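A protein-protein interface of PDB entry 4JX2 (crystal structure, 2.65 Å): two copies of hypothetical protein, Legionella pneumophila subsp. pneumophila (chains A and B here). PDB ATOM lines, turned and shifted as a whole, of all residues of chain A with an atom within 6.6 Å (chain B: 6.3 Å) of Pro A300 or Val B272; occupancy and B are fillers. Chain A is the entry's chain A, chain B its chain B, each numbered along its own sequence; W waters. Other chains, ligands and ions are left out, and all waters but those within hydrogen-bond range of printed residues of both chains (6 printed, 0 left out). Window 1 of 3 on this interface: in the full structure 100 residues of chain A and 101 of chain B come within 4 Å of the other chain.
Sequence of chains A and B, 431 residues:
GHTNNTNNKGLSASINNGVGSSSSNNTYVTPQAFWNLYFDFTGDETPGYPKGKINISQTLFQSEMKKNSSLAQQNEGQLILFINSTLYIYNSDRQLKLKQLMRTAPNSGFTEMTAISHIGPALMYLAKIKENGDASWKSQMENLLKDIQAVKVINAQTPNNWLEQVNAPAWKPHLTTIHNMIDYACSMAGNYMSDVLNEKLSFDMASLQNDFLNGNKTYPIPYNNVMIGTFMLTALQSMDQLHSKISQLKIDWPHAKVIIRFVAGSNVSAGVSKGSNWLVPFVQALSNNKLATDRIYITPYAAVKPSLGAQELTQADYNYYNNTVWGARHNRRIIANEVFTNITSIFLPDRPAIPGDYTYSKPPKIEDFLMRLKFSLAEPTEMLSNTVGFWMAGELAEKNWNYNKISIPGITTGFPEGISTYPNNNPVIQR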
ATOM      1  N   ILE A 260       7.281 -24.211 -19.599  1.00  0.00           N
ATOM      2  CA  ILE A 260       7.382 -25.662 -19.470  1.00  0.00           C
ATOM      3  C   ILE A 260       8.048 -26.001 -18.128  1.00  0.00           C
ATOM      4  O   ILE A 260       9.215 -25.683 -17.910  1.00  0.00           O
ATOM      5  CB  ILE A 260       8.104 -26.319 -20.677  1.00  0.00           C
ATOM      6  CG1 ILE A 260       7.323 -26.050 -22.002  1.00  0.00           C
ATOM      7  CG2 ILE A 260       8.316 -27.817 -20.419  1.00  0.00           C
ATOM      8  CD1 ILE A 260       8.030 -26.356 -23.283  1.00  0.00           C
ATOM      9  N   ARG A 261       7.273 -26.624 -17.234  1.00  0.00           N
ATOM     10  CA  ARG A 261       7.661 -27.149 -15.917  1.00  0.00           C
ATOM     11  C   ARG A 261       7.000 -28.536 -15.825  1.00  0.00           C
ATOM     12  O   ARG A 261       6.305 -28.873 -14.874  1.00  0.00           O
ATOM     13  CB  ARG A 261       7.246 -26.180 -14.789  1.00  0.00           C
ATOM     14  CG  ARG A 261       7.814 -26.538 -13.422  1.00  0.00           C
ATOM     15  CD  ARG A 261       6.712 -26.444 -12.390  1.00  0.00           C
ATOM     16  NE  ARG A 261       7.139 -26.843 -11.051  1.00  0.00           N
ATOM     17  CZ  ARG A 261       7.002 -28.067 -10.559  1.00  0.00           C
ATOM     18  NH1 ARG A 261       6.468 -29.028 -11.295  1.00  0.00           N
ATOM     19  NH2 ARG A 261       7.404 -28.339  -9.326  1.00  0.00           N
ATOM     20  N   PHE A 262       7.183 -29.311 -16.894  1.00  0.00           N
ATOM     21  CA  PHE A 262       6.616 -30.635 -17.082  1.00  0.00           C
ATOM     22  C   PHE A 262       7.488 -31.727 -16.448  1.00  0.00           C
ATOM     23  O   PHE A 262       8.693 -31.821 -16.723  1.00  0.00           O
ATOM     24  CB  PHE A 262       6.443 -30.890 -18.571  1.00  0.00           C
ATOM     25  CG  PHE A 262       5.761 -32.190 -18.900  1.00  0.00           C
ATOM     26  CD1 PHE A 262       4.373 -32.262 -18.987  1.00  0.00           C
ATOM     27  CD2 PHE A 262       6.505 -33.331 -19.183  1.00  0.00           C
ATOM     28  CE1 PHE A 262       3.752 -33.447 -19.349  1.00  0.00           C
ATOM     29  CE2 PHE A 262       5.878 -34.530 -19.507  1.00  0.00           C
ATOM     30  CZ  PHE A 262       4.512 -34.573 -19.609  1.00  0.00           C
ATOM     31  N   SER A 269      14.836 -35.772 -13.285  1.00  0.00           N
ATOM     32  CA  SER A 269      15.992 -35.217 -13.991  1.00  0.00           C
ATOM     33  C   SER A 269      15.784 -35.022 -15.490  1.00  0.00           C
ATOM     34  O   SER A 269      16.702 -34.554 -16.163  1.00  0.00           O
ATOM     35  CB  SER A 269      17.183 -36.149 -13.797  1.00  0.00           C
ATOM     36  OG  SER A 269      16.882 -37.444 -14.293  1.00  0.00           O
ATOM     37  N   GLY A 271      13.658 -33.973 -19.287  1.00  0.00           N
ATOM     38  CA  GLY A 271      12.930 -32.934 -20.018  1.00  0.00           C
ATOM     39  C   GLY A 271      13.098 -31.536 -19.473  1.00  0.00           C
ATOM     40  O   GLY A 271      12.132 -30.766 -19.458  1.00  0.00           O
ATOM     41  N   VAL A 272      14.321 -31.217 -18.983  1.00  0.00           N
ATOM     42  CA  VAL A 272      14.640 -29.921 -18.396  1.00  0.00           C
ATOM     43  C   VAL A 272      15.409 -29.047 -19.404  1.00  0.00           C
ATOM     44  O   VAL A 272      15.746 -27.900 -19.082  1.00  0.00           O
ATOM     45  CB  VAL A 272      15.355 -30.009 -17.018  1.00  0.00           C
ATOM     46  CG1 VAL A 272      14.441 -30.638 -15.966  1.00  0.00           C
ATOM     47  CG2 VAL A 272      16.697 -30.738 -17.103  1.00  0.00           C
ATOM     48  N   SER A 273      15.629 -29.564 -20.641  1.00  0.00           N
ATOM     49  CA  SER A 273      16.244 -28.796 -21.741  1.00  0.00           C
ATOM     50  C   SER A 273      15.485 -29.093 -23.026  1.00  0.00           C
ATOM     51  O   SER A 273      14.973 -30.194 -23.175  1.00  0.00           O
ATOM     52  CB  SER A 273      17.733 -29.069 -21.868  1.00  0.00           C
ATOM     53  OG  SER A 273      17.949 -30.429 -22.187  1.00  0.00           O
ATOM     54  N   ILE A 298      11.768 -23.154 -20.402  1.00  0.00           N
ATOM     55  CA  ILE A 298      11.704 -24.317 -19.530  1.00  0.00           C
ATOM     56  C   ILE A 298      12.141 -23.798 -18.178  1.00  0.00           C
ATOM     57  O   ILE A 298      13.304 -23.429 -18.023  1.00  0.00           O
ATOM     58  CB  ILE A 298      12.513 -25.540 -20.032  1.00  0.00           C
ATOM     59  CG1 ILE A 298      12.029 -25.966 -21.449  1.00  0.00           C
ATOM     60  CG2 ILE A 298      12.398 -26.708 -19.012  1.00  0.00           C
ATOM     61  CD1 ILE A 298      12.833 -26.931 -22.094  1.00  0.00           C
ATOM     62  N   THR A 299      11.192 -23.686 -17.234  1.00  0.00           N
ATOM     63  CA  THR A 299      11.421 -23.119 -15.912  1.00  0.00           C
ATOM     64  C   THR A 299      11.185 -24.195 -14.831  1.00  0.00           C
ATOM     65  O   THR A 299      10.151 -24.160 -14.148  1.00  0.00           O
ATOM     66  CB  THR A 299      10.519 -21.880 -15.726  1.00  0.00           C
ATOM     67  OG1 THR A 299       9.159 -22.283 -15.865  1.00  0.00           O
ATOM     68  CG2 THR A 299      10.844 -20.758 -16.717  1.00  0.00           C
ATOM     69  N   PRO A 300      12.152 -25.133 -14.613  1.00  0.00           N
ATOM     70  CA  PRO A 300      11.902 -26.224 -13.654  1.00  0.00           C
ATOM     71  C   PRO A 300      11.696 -25.792 -12.193  1.00  0.00           C
ATOM     72  O   PRO A 300      11.082 -26.537 -11.417  1.00  0.00           O
ATOM     73  CB  PRO A 300      13.142 -27.105 -13.803  1.00  0.00           C
ATOM     74  CG  PRO A 300      13.612 -26.842 -15.200  1.00  0.00           C
ATOM     75  CD  PRO A 300      13.429 -25.353 -15.316  1.00  0.00           C
ATOM     76  N   TYR A 301      12.134 -24.584 -11.839  1.00  0.00           N
ATOM     77  CA  TYR A 301      12.001 -24.135 -10.465  1.00  0.00           C
ATOM     78  C   TYR A 301      10.833 -23.160 -10.281  1.00  0.00           C
ATOM     79  O   TYR A 301      10.652 -22.628  -9.185  1.00  0.00           O
ATOM     80  CB  TYR A 301      13.330 -23.576  -9.950  1.00  0.00           C
ATOM     81  CG  TYR A 301      14.440 -24.609  -9.977  1.00  0.00           C
ATOM     82  CD1 TYR A 301      14.340 -25.797  -9.245  1.00  0.00           C
ATOM     83  CD2 TYR A 301      15.588 -24.407 -10.736  1.00  0.00           C
ATOM     84  CE1 TYR A 301      15.347 -26.762  -9.288  1.00  0.00           C
ATOM     85  CE2 TYR A 301      16.625 -25.340 -10.742  1.00  0.00           C
ATOM     86  CZ  TYR A 301      16.492 -26.528 -10.036  1.00  0.00           C
ATOM     87  OH  TYR A 301      17.522 -27.446 -10.059  1.00  0.00           O
ATOM     88  N   ALA A 302       9.983 -23.003 -11.307  1.00  0.00           N
ATOM     89  CA  ALA A 302       8.797 -22.186 -11.155  1.00  0.00           C
ATOM     90  C   ALA A 302       7.869 -22.849 -10.145  1.00  0.00           C
ATOM     91  O   ALA A 302       7.736 -24.084 -10.138  1.00  0.00           O
ATOM     92  CB  ALA A 302       8.089 -22.029 -12.487  1.00  0.00           C
ATOM     93  N   ALA A 303       7.261 -22.036  -9.268  1.00  0.00           N
ATOM     94  CA  ALA A 303       6.313 -22.517  -8.278  1.00  0.00           C
ATOM     95  C   ALA A 303       4.996 -22.982  -8.925  1.00  0.00           C
ATOM     96  O   ALA A 303       4.586 -22.458  -9.962  1.00  0.00           O
ATOM     97  CB  ALA A 303       6.019 -21.410  -7.294  1.00  0.00           C
ATOM     98  N   THR A 381      18.812 -37.155 -18.454  1.00  0.00           N
ATOM     99  CA  THR A 381      18.214 -35.981 -19.104  1.00  0.00           C
ATOM    100  C   THR A 381      16.975 -36.337 -19.933  1.00  0.00           C
ATOM    101  O   THR A 381      16.170 -35.464 -20.224  1.00  0.00           O
ATOM    102  CB  THR A 381      19.260 -35.303 -20.019  1.00  0.00           C
ATOM    103  OG1 THR A 381      19.686 -36.211 -21.053  1.00  0.00           O
ATOM    104  CG2 THR A 381      20.448 -34.786 -19.244  1.00  0.00           C
ATOM    105  N   PHE B 262      19.813 -27.001  -7.338  1.00  0.00           N
ATOM    106  CA  PHE B 262      20.219 -25.648  -6.983  1.00  0.00           C
ATOM    107  C   PHE B 262      19.419 -24.585  -7.754  1.00  0.00           C
ATOM    108  O   PHE B 262      19.361 -24.626  -8.992  1.00  0.00           O
ATOM    109  CB  PHE B 262      21.728 -25.484  -7.256  1.00  0.00           C
ATOM    110  CG  PHE B 262      22.283 -24.151  -6.810  1.00  0.00           C
ATOM    111  CD1 PHE B 262      22.662 -23.943  -5.486  1.00  0.00           C
ATOM    112  CD2 PHE B 262      22.416 -23.095  -7.713  1.00  0.00           C
ATOM    113  CE1 PHE B 262      23.137 -22.699  -5.068  1.00  0.00           C
ATOM    114  CE2 PHE B 262      22.887 -21.845  -7.291  1.00  0.00           C
ATOM    115  CZ  PHE B 262      23.265 -21.665  -5.976  1.00  0.00           C
ATOM    116  N   VAL B 268      14.538 -19.202 -12.267  1.00  0.00           N
ATOM    117  CA  VAL B 268      13.851 -20.509 -12.234  1.00  0.00           C
ATOM    118  C   VAL B 268      14.111 -21.403 -13.464  1.00  0.00           C
ATOM    119  O   VAL B 268      13.638 -22.526 -13.484  1.00  0.00           O
ATOM    120  CB  VAL B 268      12.332 -20.332 -12.016  1.00  0.00           C
ATOM    121  CG1 VAL B 268      12.042 -19.825 -10.612  1.00  0.00           C
ATOM    122  CG2 VAL B 268      11.709 -19.423 -13.074  1.00  0.00           C
ATOM    123  N   SER B 269      14.924 -20.949 -14.412  1.00  0.00           N
ATOM    124  CA  SER B 269      15.221 -21.678 -15.641  1.00  0.00           C
ATOM    125  C   SER B 269      16.722 -21.982 -15.825  1.00  0.00           C
ATOM    126  O   SER B 269      17.101 -22.600 -16.829  1.00  0.00           O
ATOM    127  CB  SER B 269      14.735 -20.852 -16.834  1.00  0.00           C
ATOM    128  OG  SER B 269      15.413 -19.605 -16.870  1.00  0.00           O
ATOM    129  N   ALA B 270      17.578 -21.518 -14.905  1.00  0.00           N
ATOM    130  CA  ALA B 270      19.033 -21.634 -15.063  1.00  0.00           C
ATOM    131  C   ALA B 270      19.668 -22.808 -14.313  1.00  0.00           C
ATOM    132  O   ALA B 270      19.070 -23.334 -13.364  1.00  0.00           O
ATOM    133  CB  ALA B 270      19.686 -20.347 -14.632  1.00  0.00           C
ATOM    134  N   GLY B 271      20.871 -23.198 -14.764  1.00  0.00           N
ATOM    135  CA  GLY B 271      21.680 -24.256 -14.169  1.00  0.00           C
ATOM    136  C   GLY B 271      20.994 -25.598 -14.017  1.00  0.00           C
ATOM    137  O   GLY B 271      21.202 -26.265 -13.012  1.00  0.00           O
ATOM    138  N   VAL B 272      20.171 -25.994 -15.002  1.00  0.00           N
ATOM    139  CA  VAL B 272      19.417 -27.246 -14.999  1.00  0.00           C
ATOM    140  C   VAL B 272      20.090 -28.291 -15.925  1.00  0.00           C
ATOM    141  O   VAL B 272      19.601 -29.424 -16.038  1.00  0.00           O
ATOM    142  CB  VAL B 272      17.905 -27.062 -15.314  1.00  0.00           C
ATOM    143  CG1 VAL B 272      17.208 -26.261 -14.222  1.00  0.00           C
ATOM    144  CG2 VAL B 272      17.668 -26.443 -16.694  1.00  0.00           C
ATOM    145  N   SER B 273      21.224 -27.929 -16.555  1.00  0.00           N
ATOM    146  CA  SER B 273      22.023 -28.850 -17.376  1.00  0.00           C
ATOM    147  C   SER B 273      23.494 -28.591 -17.066  1.00  0.00           C
ATOM    148  O   SER B 273      23.854 -27.469 -16.747  1.00  0.00           O
ATOM    149  CB  SER B 273      21.698 -28.734 -18.854  1.00  0.00           C
ATOM    150  OG  SER B 273      22.020 -27.437 -19.315  1.00  0.00           O
ATOM    151  N   LYS B 274      24.313 -29.655 -17.035  1.00  0.00           N
ATOM    152  CA  LYS B 274      25.706 -29.647 -16.595  1.00  0.00           C
ATOM    153  C   LYS B 274      26.568 -28.596 -17.283  1.00  0.00           C
ATOM    154  O   LYS B 274      27.410 -28.012 -16.611  1.00  0.00           O
ATOM    155  CB  LYS B 274      26.361 -31.037 -16.689  1.00  0.00           C
ATOM    156  CG  LYS B 274      26.288 -31.702 -18.055  1.00  0.00           C
ATOM    157  CD  LYS B 274      27.148 -32.950 -18.086  1.00  0.00           C
ATOM    158  CE  LYS B 274      27.119 -33.617 -19.435  1.00  0.00           C
ATOM    159  NZ  LYS B 274      27.652 -32.731 -20.503  1.00  0.00           N
ATOM    160  N   SER B 276      25.639 -25.695 -18.150  1.00  0.00           N
ATOM    161  CA  SER B 276      25.133 -24.393 -17.694  1.00  0.00           C
ATOM    162  C   SER B 276      25.145 -24.239 -16.154  1.00  0.00           C
ATOM    163  O   SER B 276      24.515 -23.321 -15.633  1.00  0.00           O
ATOM    164  CB  SER B 276      23.716 -24.182 -18.224  1.00  0.00           C
ATOM    165  OG  SER B 276      23.720 -24.217 -19.641  1.00  0.00           O
ATOM    166  N   ASN B 277      25.851 -25.128 -15.440  1.00  0.00           N
ATOM    167  CA  ASN B 277      25.997 -25.100 -13.981  1.00  0.00           C
ATOM    168  C   ASN B 277      27.445 -25.362 -13.611  1.00  0.00           C
ATOM    169  O   ASN B 277      27.905 -26.500 -13.698  1.00  0.00           O
ATOM    170  CB  ASN B 277      25.065 -26.099 -13.287  1.00  0.00           C
ATOM    171  CG  ASN B 277      24.801 -25.744 -11.841  1.00  0.00           C
ATOM    172  OD1 ASN B 277      25.713 -25.424 -11.068  1.00  0.00           O
ATOM    173  ND2 ASN B 277      23.536 -25.764 -11.441  1.00  0.00           N
ATOM    174  N   ILE B 298      21.671 -33.820 -11.999  1.00  0.00           N
ATOM    175  CA  ILE B 298      20.910 -32.597 -11.836  1.00  0.00           C
ATOM    176  C   ILE B 298      19.460 -33.042 -11.844  1.00  0.00           C
ATOM    177  O   ILE B 298      18.977 -33.519 -12.862  1.00  0.00           O
ATOM    178  CB  ILE B 298      21.244 -31.500 -12.891  1.00  0.00           C
ATOM    179  CG1 ILE B 298      22.745 -31.182 -12.889  1.00  0.00           C
ATOM    180  CG2 ILE B 298      20.404 -30.226 -12.635  1.00  0.00           C
ATOM    181  CD1 ILE B 298      23.179 -30.405 -14.017  1.00  0.00           C
ATOM    182  N   PRO B 300      16.089 -31.396 -11.048  1.00  0.00           N
ATOM    183  CA  PRO B 300      15.347 -30.186 -10.635  1.00  0.00           C
ATOM    184  C   PRO B 300      13.971 -30.444  -9.985  1.00  0.00           C
ATOM    185  O   PRO B 300      13.416 -29.572  -9.293  1.00  0.00           O
ATOM    186  CB  PRO B 300      15.223 -29.396 -11.946  1.00  0.00           C
ATOM    187  CG  PRO B 300      16.362 -29.847 -12.770  1.00  0.00           C
ATOM    188  CD  PRO B 300      16.446 -31.325 -12.479  1.00  0.00           C
ATOM    189  N   TYR B 301      13.425 -31.631 -10.198  1.00  0.00           N
ATOM    190  CA  TYR B 301      12.103 -31.936  -9.700  1.00  0.00           C
ATOM    191  C   TYR B 301      12.157 -32.847  -8.475  1.00  0.00           C
ATOM    192  O   TYR B 301      11.105 -33.300  -8.016  1.00  0.00           O
ATOM    193  CB  TYR B 301      11.245 -32.523 -10.826  1.00  0.00           C
ATOM    194  CG  TYR B 301      11.075 -31.570 -11.991  1.00  0.00           C
ATOM    195  CD1 TYR B 301      10.503 -30.312 -11.813  1.00  0.00           C
ATOM    196  CD2 TYR B 301      11.461 -31.935 -13.278  1.00  0.00           C
ATOM    197  CE1 TYR B 301      10.334 -29.431 -12.882  1.00  0.00           C
ATOM    198  CE2 TYR B 301      11.266 -31.073 -14.365  1.00  0.00           C
ATOM    199  CZ  TYR B 301      10.721 -29.812 -14.156  1.00  0.00           C
ATOM    200  OH  TYR B 301      10.544 -28.940 -15.212  1.00  0.00           O
ATOM    201  N   THR B 381      18.865 -20.451 -19.786  1.00  0.00           N
ATOM    202  CA  THR B 381      19.560 -21.621 -19.253  1.00  0.00           C
ATOM    203  C   THR B 381      20.732 -21.243 -18.352  1.00  0.00           C
ATOM    204  O   THR B 381      21.173 -22.063 -17.548  1.00  0.00           O
ATOM    205  CB  THR B 381      20.054 -22.490 -20.410  1.00  0.00           C
ATOM    206  OG1 THR B 381      20.961 -21.738 -21.223  1.00  0.00           O
ATOM    207  CG2 THR B 381      18.903 -23.051 -21.257  1.00  0.00           C
HETATM  208  O   HOH W   1      11.259 -27.891  -8.735  1.00  0.00           O
HETATM  209  O   HOH W   2       9.413 -30.350  -7.553  1.00  0.00           O
HETATM  210  O   HOH W   3      19.037 -33.743 -15.437  1.00  0.00           O
HETATM  211  O   HOH W   4      15.818 -23.361 -18.915  1.00  0.00           O
HETATM  212  O   HOH W   5      19.946 -26.725 -10.820  1.00  0.00           O
HETATM  213  O   HOH W   6      10.294 -29.932 -17.825  1.00  0.00           O
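Tyr B301 touches Arg A261. Ser B269 touches Ile A298. C of Thr A299 touches O of Val B268 (3.3 Å). Ser B269 touches Thr A299. Val B272 touches Pro A300. Pro A300 touches Pro B300 (CB to CB, 3.6 Å). Pro A300 touches Tyr B301 (O to CE1, 3.3 Å). O of Phe B262 touches CE2 of Tyr A301 (3.3 Å). CG1 of Val B272 touches CE2 of Tyr A301, 3.6 Å away. Pro B300 touches Tyr A301.
The backbone carbonyl oxygen (O) of Val B268 lies close to the backbone nitrogen (N) of Pro A300 (3.2 Å). N of Tyr A301 lies within hydrogen-bond range of O of Val B268 (3.0 Å).
Phe A262 touches Tyr B301, and with the chains exchanged Tyr A301 touches Phe B262. Val A272 touches Pro B300, and with the chains exchanged Pro A300 touches Val B272. Val A272 touches Tyr B301, and with the chains exchanged Tyr A301 touches Val B272. Pro A300 touches Tyr B301, and with the chains exchanged Tyr A301 touches Pro B300. Positions printed for both chains: 262, 269, 271, 272, 273, 298, 300, 301 and 381. Of the 18 pairs that touch across the chains among the printed residues, 12 have their exchanged pair printed and touching as well.
Of the printed residues of chain B, Ile A298 touches Ser B269 (3.2 Å). Of the printed residues of chain B, Thr A299 touches Val B268 (3.3 Å) and Ser B269 (3.9 Å). Pro A300 touches just these residues of chain B: Val B268 (3.2 Å), Val B272 (3.8 Å), Pro B300 (3.6 Å) and Tyr B301 (3.3 Å). Printed residues of chain A within 4 Å of Ser B269: Ile A298 and Thr A299. Of chain A, only Val A272, Pro A300 and Tyr A301 come within 4 Å of Val B272. Ser B273 touches none of the printed residues of chain A. The nearest residue of chain A that does not touch Val B272 is Ser A273 (5.4 Å). The nearest printed residue of chain A that does not touch Val B268 is Ile A298 (4.6 Å).
NE of Arg A261 lies within hydrogen-bond range of O of Ala A302 (3.0 Å). O of Ile A260 sits at hydrogen-bond distance from N of Thr A299, 2.9 Å away.
Hydrophobic or aromatic side chains of chain B that line the printed part of chain A: Val B268, Val B272, Pro B300 and Tyr B301. Of the 14 printed residues of chain A, 9 touch a printed residue of chain B. Hydrophobic or aromatic side chains of chain A that line the printed part of chain B: Val A272, Pro A300 and Tyr A301. Among the printed residues, no Asp or Glu carboxylate lies within 4 Å of a Lys or Arg side-chain nitrogen of the other chain.
Water W4 bridges the backbone carbonyl oxygen (O) of Ser B269 and the backbone carbonyl oxygen (O) of Ile A298. Water W5 lies within hydrogen-bond range of the backbone carbonyl oxygen of Gly B271 (2.6 Å), the side-chain hydroxyl of Tyr A301 (2.6 Å) and the backbone carbonyl oxygen of Phe B262 (2.8 Å). Water W3 bridges the backbone carbonyl oxygen of Ser A269 and the backbone carbonyl oxygen of Ile B298. Water W6 lies within hydrogen-bond range of O of Gly A271, O of Phe A262 and OH of Tyr B301. Water W1 bridges O of Pro B300 (2.8 Å) and O of Pro A300 (3.0 Å). Water W2 bridges NH2 of Arg A261 (3.4 Å) and O of Tyr B301 (3.4 Å).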
